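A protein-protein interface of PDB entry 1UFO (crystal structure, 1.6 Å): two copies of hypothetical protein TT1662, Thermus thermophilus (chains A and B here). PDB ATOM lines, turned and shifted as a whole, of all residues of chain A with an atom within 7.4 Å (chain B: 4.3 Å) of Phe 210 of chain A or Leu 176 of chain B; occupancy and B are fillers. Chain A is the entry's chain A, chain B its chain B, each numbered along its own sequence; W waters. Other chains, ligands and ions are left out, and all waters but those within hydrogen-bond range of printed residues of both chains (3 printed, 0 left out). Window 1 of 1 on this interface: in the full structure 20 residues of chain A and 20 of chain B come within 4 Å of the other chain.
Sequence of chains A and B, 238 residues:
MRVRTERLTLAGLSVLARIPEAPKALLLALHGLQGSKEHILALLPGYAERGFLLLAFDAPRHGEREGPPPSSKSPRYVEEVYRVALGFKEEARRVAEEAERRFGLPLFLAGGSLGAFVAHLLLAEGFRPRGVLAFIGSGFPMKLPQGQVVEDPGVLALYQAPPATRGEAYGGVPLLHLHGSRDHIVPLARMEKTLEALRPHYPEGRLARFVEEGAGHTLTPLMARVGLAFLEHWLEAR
OE1 of Glu 213 of chain A is in salt-bridge range of NH1 of Arg 209 of chain B (3.0 Å). O of Val 211 of chain A is in hydrogen-bond range of N of Arg 209 of chain B (2.9 Å).
Ser 181 of chain A touches none of the printed residues of chain B. Phe 210 of chain A touches just these residues of chain B: Leu 176, Ala 208 and Arg 209. Printed residues of chain B within 4 Å of Val 211 of chain A: Ala 208 and Arg 209. Of the printed residues of chain B, Leu 222 of chain A touches Phe 230 (3.9 Å). Leu 176 of chain B touches just one residue of chain A: Phe 210. Of the printed residues of chain A, Phe 230 of chain B touches Leu 222 (3.9 Å).
Among the printed residues, merely in contact across the chains: Leu 176 of chain A with Phe 210 of chain B (3.99 Å), Ala 208 of chain A with Phe 210 of chain B (3.7 Å), Arg 209 of chain A with Phe 210 of chain B (3.3 Å), Phe 210 of chain A with Leu 176 of chain B (3.9 Å), Phe 210 of chain A with Ala 208 of chain B (3.6 Å), Phe 210 of chain A with Arg 209 of chain B (3.3 Å), Val 211 of chain A with Ala 208 of chain B (3.3 Å), Leu 222 of chain A with Phe 230 of chain B (3.9 Å) and Val 226 of chain A with Val 226 of chain B (3.9 Å).
Of the 23 printed residues of chain A, 8 touch a printed residue of chain B. Printed residues of chain A that touch a printed residue of chain B: Leu 176, Ala 208, Arg 209, Phe 210, Val 211, Glu 213, Leu 222 and Val 226. Hydrophobic or aromatic side chains of chain A that line the printed part of chain B: Leu 176, Ala 208, Phe 210, Val 211, Leu 222 and Val 226. Hydrophobic or aromatic side chains of chain B that line the printed part of chain A: Leu 176, Ala 208, Phe 210, Val 226 and Phe 230. Among the printed residues, Asp or Glu carboxylates within 4 Å of a Lys or Arg side-chain nitrogen of the other chain: Glu 213 of chain A with Arg 209 of chain B (3.0 Å).
Leu 176 of chain A touches Phe 210 of chain B, and with the chains exchanged Phe 210 of chain A touches Leu 176 of chain B. Ala 208 of chain A touches Phe 210 of chain B, and with the chains exchanged Phe 210 of chain A touches Ala 208 of chain B. Arg 209 of chain A touches Phe 210 of chain B, and with the chains exchanged Phe 210 of chain A touches Arg 209 of chain B. Val 226 of chain B touches its own counterpart, Val 226 of chain A.
Water W1 lies within hydrogen-bond range of OE1 of Glu 213 of chain A, NE of Arg 209 of chain B and O of Val 211 of chain A. Water W2 lies within hydrogen-bond range of OE2 of Glu 213 of chain A (2.9 Å) and NH1 of Arg 209 of chain B (3.4 Å). Water W3 bridges the side-chain carboxylate (OE1) of Glu 213 of chain A and the guanidinium group (NH1) of Arg 209 of chain B.
O of His 177 of chain B sits at hydrogen-bond distance from N of Phe 210 of chain B, at 2.8 Å. The backbone carbonyl oxygen (O) of Leu 176 of chain B is in hydrogen-bond range of the backbone NH (N) of Ala 134 of chain B (2.8 Å). The backbone carbonyl oxygen (O) of Phe 210 of chain A sits at hydrogen-bond distance from the backbone NH (N) of His 179 of chain A, 2.8 Å away. The backbone carbonyl oxygen (O) of Ala 208 of chain B is in hydrogen-bond range of the backbone NH (N) of His 177 of chain B. The backbone carbonyl oxygen (O) of His 177 of chain A is in hydrogen-bond range of the backbone NH (N) of Phe 210 of chain A (2.8 Å). The backbone carbonyl oxygen of Val 132 of chain B lies within hydrogen-bond range of the backbone NH of Leu 176 of chain B (3.1 Å).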
ATOM      1  N   ALA A 134     -14.543  29.244 -28.745  1.00  0.00           N
ATOM      2  CA  ALA A 134     -15.152  30.350 -28.022  1.00  0.00           C
ATOM      3  C   ALA A 134     -15.812  29.716 -26.795  1.00  0.00           C
ATOM      4  O   ALA A 134     -16.887  29.103 -26.860  1.00  0.00           O
ATOM      5  CB  ALA A 134     -16.230  31.038 -28.949  1.00  0.00           C
ATOM      6  N   PHE A 135     -15.116  29.878 -25.647  1.00  0.00           N
ATOM      7  CA  PHE A 135     -15.603  29.306 -24.422  1.00  0.00           C
ATOM      8  C   PHE A 135     -16.433  30.332 -23.643  1.00  0.00           C
ATOM      9  O   PHE A 135     -16.063  31.487 -23.577  1.00  0.00           O
ATOM     10  CB  PHE A 135     -14.444  28.960 -23.506  1.00  0.00           C
ATOM     11  CG  PHE A 135     -13.591  27.840 -23.977  1.00  0.00           C
ATOM     12  CD1 PHE A 135     -12.403  28.089 -24.699  1.00  0.00           C
ATOM     13  CD2 PHE A 135     -13.900  26.496 -23.629  1.00  0.00           C
ATOM     14  CE1 PHE A 135     -11.554  27.048 -25.054  1.00  0.00           C
ATOM     15  CE2 PHE A 135     -13.060  25.459 -23.978  1.00  0.00           C
ATOM     16  CZ  PHE A 135     -11.860  25.714 -24.701  1.00  0.00           C
ATOM     17  N   LEU A 176     -16.104  26.747 -32.760  1.00  0.00           N
ATOM     18  CA  LEU A 176     -16.871  25.934 -31.787  1.00  0.00           C
ATOM     19  C   LEU A 176     -17.182  26.766 -30.566  1.00  0.00           C
ATOM     20  O   LEU A 176     -16.257  27.325 -29.986  1.00  0.00           O
ATOM     21  CB  LEU A 176     -16.056  24.681 -31.315  1.00  0.00           C
ATOM     22  CG  LEU A 176     -16.612  23.972 -30.115  1.00  0.00           C
ATOM     23  CD1 LEU A 176     -18.015  23.422 -30.557  1.00  0.00           C
ATOM     24  CD2 LEU A 176     -15.678  22.824 -29.735  1.00  0.00           C
ATOM     25  N   HIS A 177     -18.463  26.891 -30.215  1.00  0.00           N
ATOM     26  CA  HIS A 177     -18.843  27.609 -28.987  1.00  0.00           C
ATOM     27  C   HIS A 177     -19.052  26.514 -27.927  1.00  0.00           C
ATOM     28  O   HIS A 177     -19.731  25.513 -28.168  1.00  0.00           O
ATOM     29  CB  HIS A 177     -20.136  28.419 -29.164  1.00  0.00           C
ATOM     30  CG  HIS A 177     -19.921  29.870 -29.362  1.00  0.00           C
ATOM     31  ND1 HIS A 177     -19.787  30.750 -28.296  1.00  0.00           N
ATOM     32  CD2 HIS A 177     -19.745  30.629 -30.491  1.00  0.00           C
ATOM     33  CE1 HIS A 177     -19.554  31.976 -28.771  1.00  0.00           C
ATOM     34  NE2 HIS A 177     -19.514  31.913 -30.096  1.00  0.00           N
ATOM     35  N   LEU A 178     -18.414  26.684 -26.756  1.00  0.00           N
ATOM     36  CA  LEU A 178     -18.546  25.703 -25.673  1.00  0.00           C
ATOM     37  C   LEU A 178     -19.205  26.486 -24.532  1.00  0.00           C
ATOM     38  O   LEU A 178     -18.757  27.597 -24.185  1.00  0.00           O
ATOM     39  CB  LEU A 178     -17.155  25.183 -25.204  1.00  0.00           C
ATOM     40  CG  LEU A 178     -16.419  24.551 -26.395  1.00  0.00           C
ATOM     41  CD1 LEU A 178     -15.368  25.527 -27.017  1.00  0.00           C
ATOM     42  CD2 LEU A 178     -15.673  23.277 -25.856  1.00  0.00           C
ATOM     43  N   HIS A 179     -20.283  25.943 -23.950  1.00  0.00           N
ATOM     44  CA  HIS A 179     -21.028  26.712 -22.945  1.00  0.00           C
ATOM     45  C   HIS A 179     -21.640  25.820 -21.882  1.00  0.00           C
ATOM     46  O   HIS A 179     -21.770  24.619 -22.066  1.00  0.00           O
ATOM     47  CB  HIS A 179     -22.220  27.371 -23.664  1.00  0.00           C
ATOM     48  CG  HIS A 179     -22.507  28.777 -23.253  1.00  0.00           C
ATOM     49  ND1 HIS A 179     -21.839  29.854 -23.826  1.00  0.00           N
ATOM     50  CD2 HIS A 179     -23.370  29.310 -22.338  1.00  0.00           C
ATOM     51  CE1 HIS A 179     -22.260  30.983 -23.277  1.00  0.00           C
ATOM     52  NE2 HIS A 179     -23.199  30.684 -22.368  1.00  0.00           N
ATOM     53  N   GLY A 180     -21.983  26.462 -20.760  1.00  0.00           N
ATOM     54  CA  GLY A 180     -22.663  25.736 -19.673  1.00  0.00           C
ATOM     55  C   GLY A 180     -24.124  26.140 -19.708  1.00  0.00           C
ATOM     56  O   GLY A 180     -24.473  27.310 -19.845  1.00  0.00           O
ATOM     57  N   SER A 181     -25.027  25.181 -19.532  1.00  0.00           N
ATOM     58  CA  SER A 181     -26.450  25.541 -19.632  1.00  0.00           C
ATOM     59  C   SER A 181     -26.964  26.511 -18.579  1.00  0.00           C
ATOM     60  O   SER A 181     -27.993  27.195 -18.846  1.00  0.00           O
ATOM     61  CB  SER A 181     -27.308  24.260 -19.613  1.00  0.00           C
ATOM     62  OG  SER A 181     -27.270  23.645 -18.320  1.00  0.00           O
ATOM     63  N   LEU A 188     -27.171  31.201 -21.990  1.00  0.00           N
ATOM     64  CA  LEU A 188     -27.145  30.281 -23.115  1.00  0.00           C
ATOM     65  C   LEU A 188     -27.791  30.847 -24.363  1.00  0.00           C
ATOM     66  O   LEU A 188     -27.278  30.674 -25.500  1.00  0.00           O
ATOM     67  CB  LEU A 188     -27.811  28.950 -22.732  1.00  0.00           C
ATOM     68  CG  LEU A 188     -27.820  27.862 -23.822  1.00  0.00           C
ATOM     69  CD1 LEU A 188     -26.399  27.361 -23.965  1.00  0.00           C
ATOM     70  CD2 LEU A 188     -28.741  26.696 -23.432  1.00  0.00           C
ATOM     71  N   MET A 191     -25.419  32.788 -26.707  1.00  0.00           N
ATOM     72  CA  MET A 191     -24.592  31.936 -27.525  1.00  0.00           C
ATOM     73  C   MET A 191     -25.426  31.380 -28.662  1.00  0.00           C
ATOM     74  O   MET A 191     -25.019  31.352 -29.787  1.00  0.00           O
ATOM     75  CB  MET A 191     -24.028  30.795 -26.678  1.00  0.00           C
ATOM     76  CG  MET A 191     -23.105  29.825 -27.510  1.00  0.00           C
ATOM     77  SD  MET A 191     -24.069  28.440 -28.466  1.00  0.00           S
ATOM     78  CE  MET A 191     -23.906  27.387 -26.992  1.00  0.00           C
ATOM     79  N   LEU A 195     -24.864  31.834 -32.893  1.00  0.00           N
ATOM     80  CA  LEU A 195     -24.820  30.819 -33.900  1.00  0.00           C
ATOM     81  C   LEU A 195     -25.910  30.988 -34.943  1.00  0.00           C
ATOM     82  O   LEU A 195     -25.681  30.730 -36.054  1.00  0.00           O
ATOM     83  CB  LEU A 195     -24.898  29.435 -33.261  1.00  0.00           C
ATOM     84  CG  LEU A 195     -23.537  28.726 -33.077  1.00  0.00           C
ATOM     85  CD1 LEU A 195     -22.493  29.493 -32.399  1.00  0.00           C
ATOM     86  CD2 LEU A 195     -23.837  27.526 -32.289  1.00  0.00           C
ATOM     87  N   ALA A 208     -20.050  24.853 -34.757  1.00  0.00           N
ATOM     88  CA  ALA A 208     -20.566  23.825 -33.846  1.00  0.00           C
ATOM     89  C   ALA A 208     -20.728  24.382 -32.434  1.00  0.00           C
ATOM     90  O   ALA A 208     -20.216  25.447 -32.098  1.00  0.00           O
ATOM     91  CB  ALA A 208     -19.602  22.574 -33.805  1.00  0.00           C
ATOM     92  N   ARG A 209     -21.517  23.636 -31.643  1.00  0.00           N
ATOM     93  CA  ARG A 209     -21.684  24.007 -30.223  1.00  0.00           C
ATOM     94  C   ARG A 209     -21.542  22.806 -29.324  1.00  0.00           C
ATOM     95  O   ARG A 209     -21.828  21.649 -29.702  1.00  0.00           O
ATOM     96  CB  ARG A 209     -23.071  24.679 -29.964  1.00  0.00           C
ATOM     97  CG  ARG A 209     -24.285  23.826 -30.222  1.00  0.00           C
ATOM     98  CD  ARG A 209     -25.634  24.708 -30.169  1.00  0.00           C
ATOM     99  NE  ARG A 209     -26.235  24.856 -31.473  1.00  0.00           N
ATOM    100  CZ  ARG A 209     -27.391  24.314 -31.901  1.00  0.00           C
ATOM    101  NH1 ARG A 209     -27.806  24.566 -33.153  1.00  0.00           N
ATOM    102  NH2 ARG A 209     -28.153  23.548 -31.116  1.00  0.00           N
ATOM    103  N   PHE A 210     -21.055  23.032 -28.107  1.00  0.00           N
ATOM    104  CA  PHE A 210     -20.939  21.987 -27.110  1.00  0.00           C
ATOM    105  C   PHE A 210     -21.516  22.622 -25.860  1.00  0.00           C
ATOM    106  O   PHE A 210     -21.075  23.708 -25.448  1.00  0.00           O
ATOM    107  CB  PHE A 210     -19.468  21.600 -26.821  1.00  0.00           C
ATOM    108  CG  PHE A 210     -19.342  20.704 -25.632  1.00  0.00           C
ATOM    109  CD1 PHE A 210     -19.697  19.350 -25.752  1.00  0.00           C
ATOM    110  CD2 PHE A 210     -18.908  21.220 -24.394  1.00  0.00           C
ATOM    111  CE1 PHE A 210     -19.636  18.445 -24.641  1.00  0.00           C
ATOM    112  CE2 PHE A 210     -18.862  20.318 -23.287  1.00  0.00           C
ATOM    113  CZ  PHE A 210     -19.230  18.947 -23.431  1.00  0.00           C
ATOM    114  N   VAL A 211     -22.548  21.965 -25.294  1.00  0.00           N
ATOM    115  CA  VAL A 211     -23.154  22.488 -24.086  1.00  0.00           C
ATOM    116  C   VAL A 211     -23.093  21.431 -22.996  1.00  0.00           C
ATOM    117  O   VAL A 211     -23.533  20.271 -23.192  1.00  0.00           O
ATOM    118  CB  VAL A 211     -24.644  22.919 -24.315  1.00  0.00           C
ATOM    119  CG1 VAL A 211     -25.227  23.510 -22.977  1.00  0.00           C
ATOM    120  CG2 VAL A 211     -24.728  24.013 -25.402  1.00  0.00           C
ATOM    121  N   GLU A 212     -22.511  21.798 -21.865  1.00  0.00           N
ATOM    122  CA  GLU A 212     -22.391  20.906 -20.692  1.00  0.00           C
ATOM    123  C   GLU A 212     -23.601  21.255 -19.791  1.00  0.00           C
ATOM    124  O   GLU A 212     -23.740  22.390 -19.297  1.00  0.00           O
ATOM    125  CB  GLU A 212     -21.078  21.194 -20.014  1.00  0.00           C
ATOM    126  CG  GLU A 212     -20.808  20.333 -18.784  1.00  0.00           C
ATOM    127  CD  GLU A 212     -19.393  20.511 -18.281  1.00  0.00           C
ATOM    128  OE1 GLU A 212     -19.167  20.249 -17.096  1.00  0.00           O
ATOM    129  OE2 GLU A 212     -18.558  20.969 -19.052  1.00  0.00           O
ATOM    130  N   GLU A 213     -24.449  20.254 -19.552  1.00  0.00           N
ATOM    131  CA  GLU A 213     -25.675  20.513 -18.787  1.00  0.00           C
ATOM    132  C   GLU A 213     -25.291  20.727 -17.323  1.00  0.00           C
ATOM    133  O   GLU A 213     -24.567  19.893 -16.735  1.00  0.00           O
ATOM    134  CB  GLU A 213     -26.564  19.297 -18.922  1.00  0.00           C
ATOM    135  CG  GLU A 213     -27.992  19.662 -18.737  1.00  0.00           C
ATOM    136  CD  GLU A 213     -28.564  20.555 -19.848  1.00  0.00           C
ATOM    137  OE1 GLU A 213     -28.061  20.678 -21.027  1.00  0.00           O
ATOM    138  OE2 GLU A 213     -29.645  21.097 -19.551  1.00  0.00           O
ATOM    139  N   THR A 220     -14.794  24.510 -17.978  1.00  0.00           N
ATOM    140  CA  THR A 220     -14.637  23.212 -17.269  1.00  0.00           C
ATOM    141  C   THR A 220     -13.652  22.292 -17.951  1.00  0.00           C
ATOM    142  O   THR A 220     -13.378  22.409 -19.157  1.00  0.00           O
ATOM    143  CB  THR A 220     -15.961  22.407 -17.207  1.00  0.00           C
ATOM    144  OG1 THR A 220     -16.327  22.052 -18.557  1.00  0.00           O
ATOM    145  CG2 THR A 220     -17.050  23.243 -16.624  1.00  0.00           C
ATOM    146  N   LEU A 222     -14.132  19.309 -18.881  1.00  0.00           N
ATOM    147  CA  LEU A 222     -14.780  18.600 -20.015  1.00  0.00           C
ATOM    148  C   LEU A 222     -14.829  19.524 -21.275  1.00  0.00           C
ATOM    149  O   LEU A 222     -14.561  19.079 -22.389  1.00  0.00           O
ATOM    150  CB  LEU A 222     -16.205  18.149 -19.661  1.00  0.00           C
ATOM    151  CG  LEU A 222     -16.916  17.419 -20.811  1.00  0.00           C
ATOM    152  CD1 LEU A 222     -16.178  16.162 -21.330  1.00  0.00           C
ATOM    153  CD2 LEU A 222     -18.325  17.013 -20.336  1.00  0.00           C
ATOM    154  N   MET A 223     -15.167  20.803 -21.094  1.00  0.00           N
ATOM    155  CA  MET A 223     -15.120  21.739 -22.218  1.00  0.00           C
ATOM    156  C   MET A 223     -13.710  21.780 -22.796  1.00  0.00           C
ATOM    157  O   MET A 223     -13.545  21.780 -23.991  1.00  0.00           O
ATOM    158  CB  MET A 223     -15.511  23.142 -21.716  1.00  0.00           C
ATOM    159  CG  MET A 223     -17.019  23.378 -21.491  1.00  0.00           C
ATOM    160  SD  MET A 223     -17.233  25.121 -20.759  1.00  0.00           S
ATOM    161  CE  MET A 223     -18.936  24.794 -19.804  1.00  0.00           C
ATOM    162  N   ALA A 224     -12.684  21.824 -21.957  1.00  0.00           N
ATOM    163  CA  ALA A 224     -11.355  21.900 -22.536  1.00  0.00           C
ATOM    164  C   ALA A 224     -11.042  20.704 -23.366  1.00  0.00           C
ATOM    165  O   ALA A 224     -10.436  20.814 -24.413  1.00  0.00           O
ATOM    166  CB  ALA A 224     -10.328  22.062 -21.380  1.00  0.00           C
ATOM    167  N   VAL A 226     -13.128  18.713 -24.968  1.00  0.00           N
ATOM    168  CA  VAL A 226     -13.855  18.719 -26.244  1.00  0.00           C
ATOM    169  C   VAL A 226     -13.232  19.740 -27.228  1.00  0.00           C
ATOM    170  O   VAL A 226     -13.136  19.523 -28.430  1.00  0.00           O
ATOM    171  CB  VAL A 226     -15.349  19.028 -25.990  1.00  0.00           C
ATOM    172  CG1 VAL A 226     -16.064  19.282 -27.288  1.00  0.00           C
ATOM    173  CG2 VAL A 226     -15.954  17.824 -25.279  1.00  0.00           C
ATOM    174  N   GLY A 227     -12.775  20.871 -26.683  1.00  0.00           N
ATOM    175  CA  GLY A 227     -12.185  21.884 -27.533  1.00  0.00           C
ATOM    176  C   GLY A 227     -10.877  21.357 -28.154  1.00  0.00           C
ATOM    177  O   GLY A 227     -10.600  21.708 -29.301  1.00  0.00           O
ATOM    178  N   VAL B 132     -21.616   6.702 -22.238  1.00  0.00           N
ATOM    179  CA  VAL B 132     -22.380   6.423 -23.441  1.00  0.00           C
ATOM    180  C   VAL B 132     -22.276   7.561 -24.466  1.00  0.00           C
ATOM    181  O   VAL B 132     -22.404   8.753 -24.083  1.00  0.00           O
ATOM    182  CB  VAL B 132     -23.890   6.291 -23.054  1.00  0.00           C
ATOM    183  CG1 VAL B 132     -24.768   6.106 -24.347  1.00  0.00           C
ATOM    184  CG2 VAL B 132     -24.033   5.064 -22.119  1.00  0.00           C
ATOM    185  N   LEU B 133     -22.038   7.194 -25.723  1.00  0.00           N
ATOM    186  CA  LEU B 133     -22.094   8.211 -26.802  1.00  0.00           C
ATOM    187  C   LEU B 133     -23.386   7.904 -27.566  1.00  0.00           C
ATOM    188  O   LEU B 133     -23.609   6.793 -28.076  1.00  0.00           O
ATOM    189  CB  LEU B 133     -20.938   8.044 -27.834  1.00  0.00           C
ATOM    190  CG  LEU B 133     -19.572   8.139 -27.202  1.00  0.00           C
ATOM    191  CD1 LEU B 133     -18.532   7.871 -28.320  1.00  0.00           C
ATOM    192  CD2 LEU B 133     -19.347   9.532 -26.566  1.00  0.00           C
ATOM    193  N   ALA B 134     -24.270   8.907 -27.668  1.00  0.00           N
ATOM    194  CA  ALA B 134     -25.480   8.727 -28.441  1.00  0.00           C
ATOM    195  C   ALA B 134     -25.414   9.637 -29.656  1.00  0.00           C
ATOM    196  O   ALA B 134     -25.589  10.850 -29.553  1.00  0.00           O
ATOM    197  CB  ALA B 134     -26.723   9.074 -27.573  1.00  0.00           C
ATOM    198  N   LEU B 175     -23.173  10.729 -20.334  1.00  0.00           N
ATOM    199  CA  LEU B 175     -23.870  10.622 -21.592  1.00  0.00           C
ATOM    200  C   LEU B 175     -23.648  11.886 -22.408  1.00  0.00           C
ATOM    201  O   LEU B 175     -23.887  12.991 -21.935  1.00  0.00           O
ATOM    202  CB  LEU B 175     -25.408  10.458 -21.273  1.00  0.00           C
ATOM    203  CG  LEU B 175     -26.331  10.478 -22.511  1.00  0.00           C
ATOM    204  CD1 LEU B 175     -26.090   9.405 -23.463  1.00  0.00           C
ATOM    205  CD2 LEU B 175     -27.749  10.430 -21.973  1.00  0.00           C
ATOM    206  N   LEU B 176     -23.190  11.670 -23.646  1.00  0.00           N
ATOM    207  CA  LEU B 176     -23.011  12.759 -24.617  1.00  0.00           C
ATOM    208  C   LEU B 176     -23.868  12.430 -25.877  1.00  0.00           C
ATOM    209  O   LEU B 176     -23.724  11.321 -26.464  1.00  0.00           O
ATOM    210  CB  LEU B 176     -21.539  12.836 -25.037  1.00  0.00           C
ATOM    211  CG  LEU B 176     -21.279  13.819 -26.196  1.00  0.00           C
ATOM    212  CD1 LEU B 176     -21.598  15.269 -25.754  1.00  0.00           C
ATOM    213  CD2 LEU B 176     -19.854  13.775 -26.649  1.00  0.00           C
ATOM    214  N   HIS B 177     -24.780  13.366 -26.222  1.00  0.00           N
ATOM    215  CA  HIS B 177     -25.529  13.283 -27.470  1.00  0.00           C
ATOM    216  C   HIS B 177     -24.800  14.124 -28.520  1.00  0.00           C
ATOM    217  O   HIS B 177     -24.400  15.259 -28.225  1.00  0.00           O
ATOM    218  CB  HIS B 177     -26.977  13.844 -27.299  1.00  0.00           C
ATOM    219  CG  HIS B 177     -27.996  12.755 -27.137  1.00  0.00           C
ATOM    220  ND1 HIS B 177     -28.629  12.181 -28.229  1.00  0.00           N
ATOM    221  CD2 HIS B 177     -28.456  12.115 -26.041  1.00  0.00           C
ATOM    222  CE1 HIS B 177     -29.436  11.213 -27.787  1.00  0.00           C
ATOM    223  NE2 HIS B 177     -29.345  11.156 -26.470  1.00  0.00           N
ATOM    224  N   LEU B 178     -24.606  13.539 -29.712  1.00  0.00           N
ATOM    225  CA  LEU B 178     -23.912  14.257 -30.805  1.00  0.00           C
ATOM    226  C   LEU B 178     -24.916  14.302 -31.922  1.00  0.00           C
ATOM    227  O   LEU B 178     -25.477  13.238 -32.284  1.00  0.00           O
ATOM    228  CB  LEU B 178     -22.644  13.526 -31.228  1.00  0.00           C
ATOM    229  CG  LEU B 178     -21.657  13.311 -30.040  1.00  0.00           C
ATOM    230  CD1 LEU B 178     -21.801  11.936 -29.472  1.00  0.00           C
ATOM    231  CD2 LEU B 178     -20.189  13.495 -30.496  1.00  0.00           C
ATOM    232  N   ALA B 208     -24.142  15.967 -21.541  1.00  0.00           N
ATOM    233  CA  ALA B 208     -23.783  17.033 -22.484  1.00  0.00           C
ATOM    234  C   ALA B 208     -24.244  16.782 -23.896  1.00  0.00           C
ATOM    235  O   ALA B 208     -24.677  15.679 -24.240  1.00  0.00           O
ATOM    236  CB  ALA B 208     -22.189  17.203 -22.462  1.00  0.00           C
ATOM    237  N   ARG B 209     -24.142  17.839 -24.728  1.00  0.00           N
ATOM    238  CA  ARG B 209     -24.539  17.665 -26.128  1.00  0.00           C
ATOM    239  C   ARG B 209     -23.535  18.364 -27.028  1.00  0.00           C
ATOM    240  O   ARG B 209     -22.940  19.366 -26.611  1.00  0.00           O
ATOM    241  CB  ARG B 209     -25.948  18.271 -26.385  1.00  0.00           C
ATOM    242  CG  ARG B 209     -25.925  19.817 -26.317  1.00  0.00           C
ATOM    243  CD  ARG B 209     -27.378  20.385 -26.282  1.00  0.00           C
ATOM    244  NE  ARG B 209     -27.946  20.281 -24.988  1.00  0.00           N
ATOM    245  CZ  ARG B 209     -29.232  20.527 -24.771  1.00  0.00           C
ATOM    246  NH1 ARG B 209     -29.684  20.403 -23.545  1.00  0.00           N
ATOM    247  NH2 ARG B 209     -30.045  20.879 -25.791  1.00  0.00           N
ATOM    248  N   PHE B 210     -23.337  17.801 -28.217  1.00  0.00           N
ATOM    249  CA  PHE B 210     -22.454  18.431 -29.232  1.00  0.00           C
ATOM    250  C   PHE B 210     -23.293  18.554 -30.501  1.00  0.00           C
ATOM    251  O   PHE B 210     -23.896  17.519 -30.917  1.00  0.00           O
ATOM    252  CB  PHE B 210     -21.207  17.591 -29.516  1.00  0.00           C
ATOM    253  CG  PHE B 210     -20.380  18.066 -30.670  1.00  0.00           C
ATOM    254  CD1 PHE B 210     -19.458  19.127 -30.520  1.00  0.00           C
ATOM    255  CD2 PHE B 210     -20.549  17.507 -31.928  1.00  0.00           C
ATOM    256  CE1 PHE B 210     -18.698  19.628 -31.599  1.00  0.00           C
ATOM    257  CE2 PHE B 210     -19.801  17.985 -33.048  1.00  0.00           C
ATOM    258  CZ  PHE B 210     -18.858  19.071 -32.860  1.00  0.00           C
ATOM    259  N   VAL B 226     -14.962  14.097 -31.370  1.00  0.00           N
ATOM    260  CA  VAL B 226     -15.476  14.617 -30.115  1.00  0.00           C
ATOM    261  C   VAL B 226     -15.911  13.469 -29.162  1.00  0.00           C
ATOM    262  O   VAL B 226     -15.600  13.471 -28.002  1.00  0.00           O
ATOM    263  CB  VAL B 226     -16.663  15.561 -30.409  1.00  0.00           C
ATOM    264  CG1 VAL B 226     -17.307  15.998 -29.056  1.00  0.00           C
ATOM    265  CG2 VAL B 226     -16.101  16.859 -31.065  1.00  0.00           C
ATOM    266  N   PHE B 230     -14.586  12.442 -25.353  1.00  0.00           N
ATOM    267  CA  PHE B 230     -15.504  12.284 -24.236  1.00  0.00           C
ATOM    268  C   PHE B 230     -15.253  10.923 -23.528  1.00  0.00           C
ATOM    269  O   PHE B 230     -15.236  10.903 -22.308  1.00  0.00           O
ATOM    270  CB  PHE B 230     -16.973  12.366 -24.757  1.00  0.00           C
ATOM    271  CG  PHE B 230     -18.032  12.313 -23.659  1.00  0.00           C
ATOM    272  CD1 PHE B 230     -18.411  13.475 -23.006  1.00  0.00           C
ATOM    273  CD2 PHE B 230     -18.698  11.099 -23.289  1.00  0.00           C
ATOM    274  CE1 PHE B 230     -19.416  13.500 -22.053  1.00  0.00           C
ATOM    275  CE2 PHE B 230     -19.739  11.176 -22.275  1.00  0.00           C
ATOM    276  CZ  PHE B 230     -20.079  12.356 -21.696  1.00  0.00           C
HETATM  277  O   HOH W   1     -26.320  19.670 -22.771  1.00  0.00           O
HETATM  278  O   HOH W   2     -32.009  21.110 -21.200  1.00  0.00           O
HETATM  279  O   HOH W   3     -28.791  23.368 -22.303  1.00  0.00           O
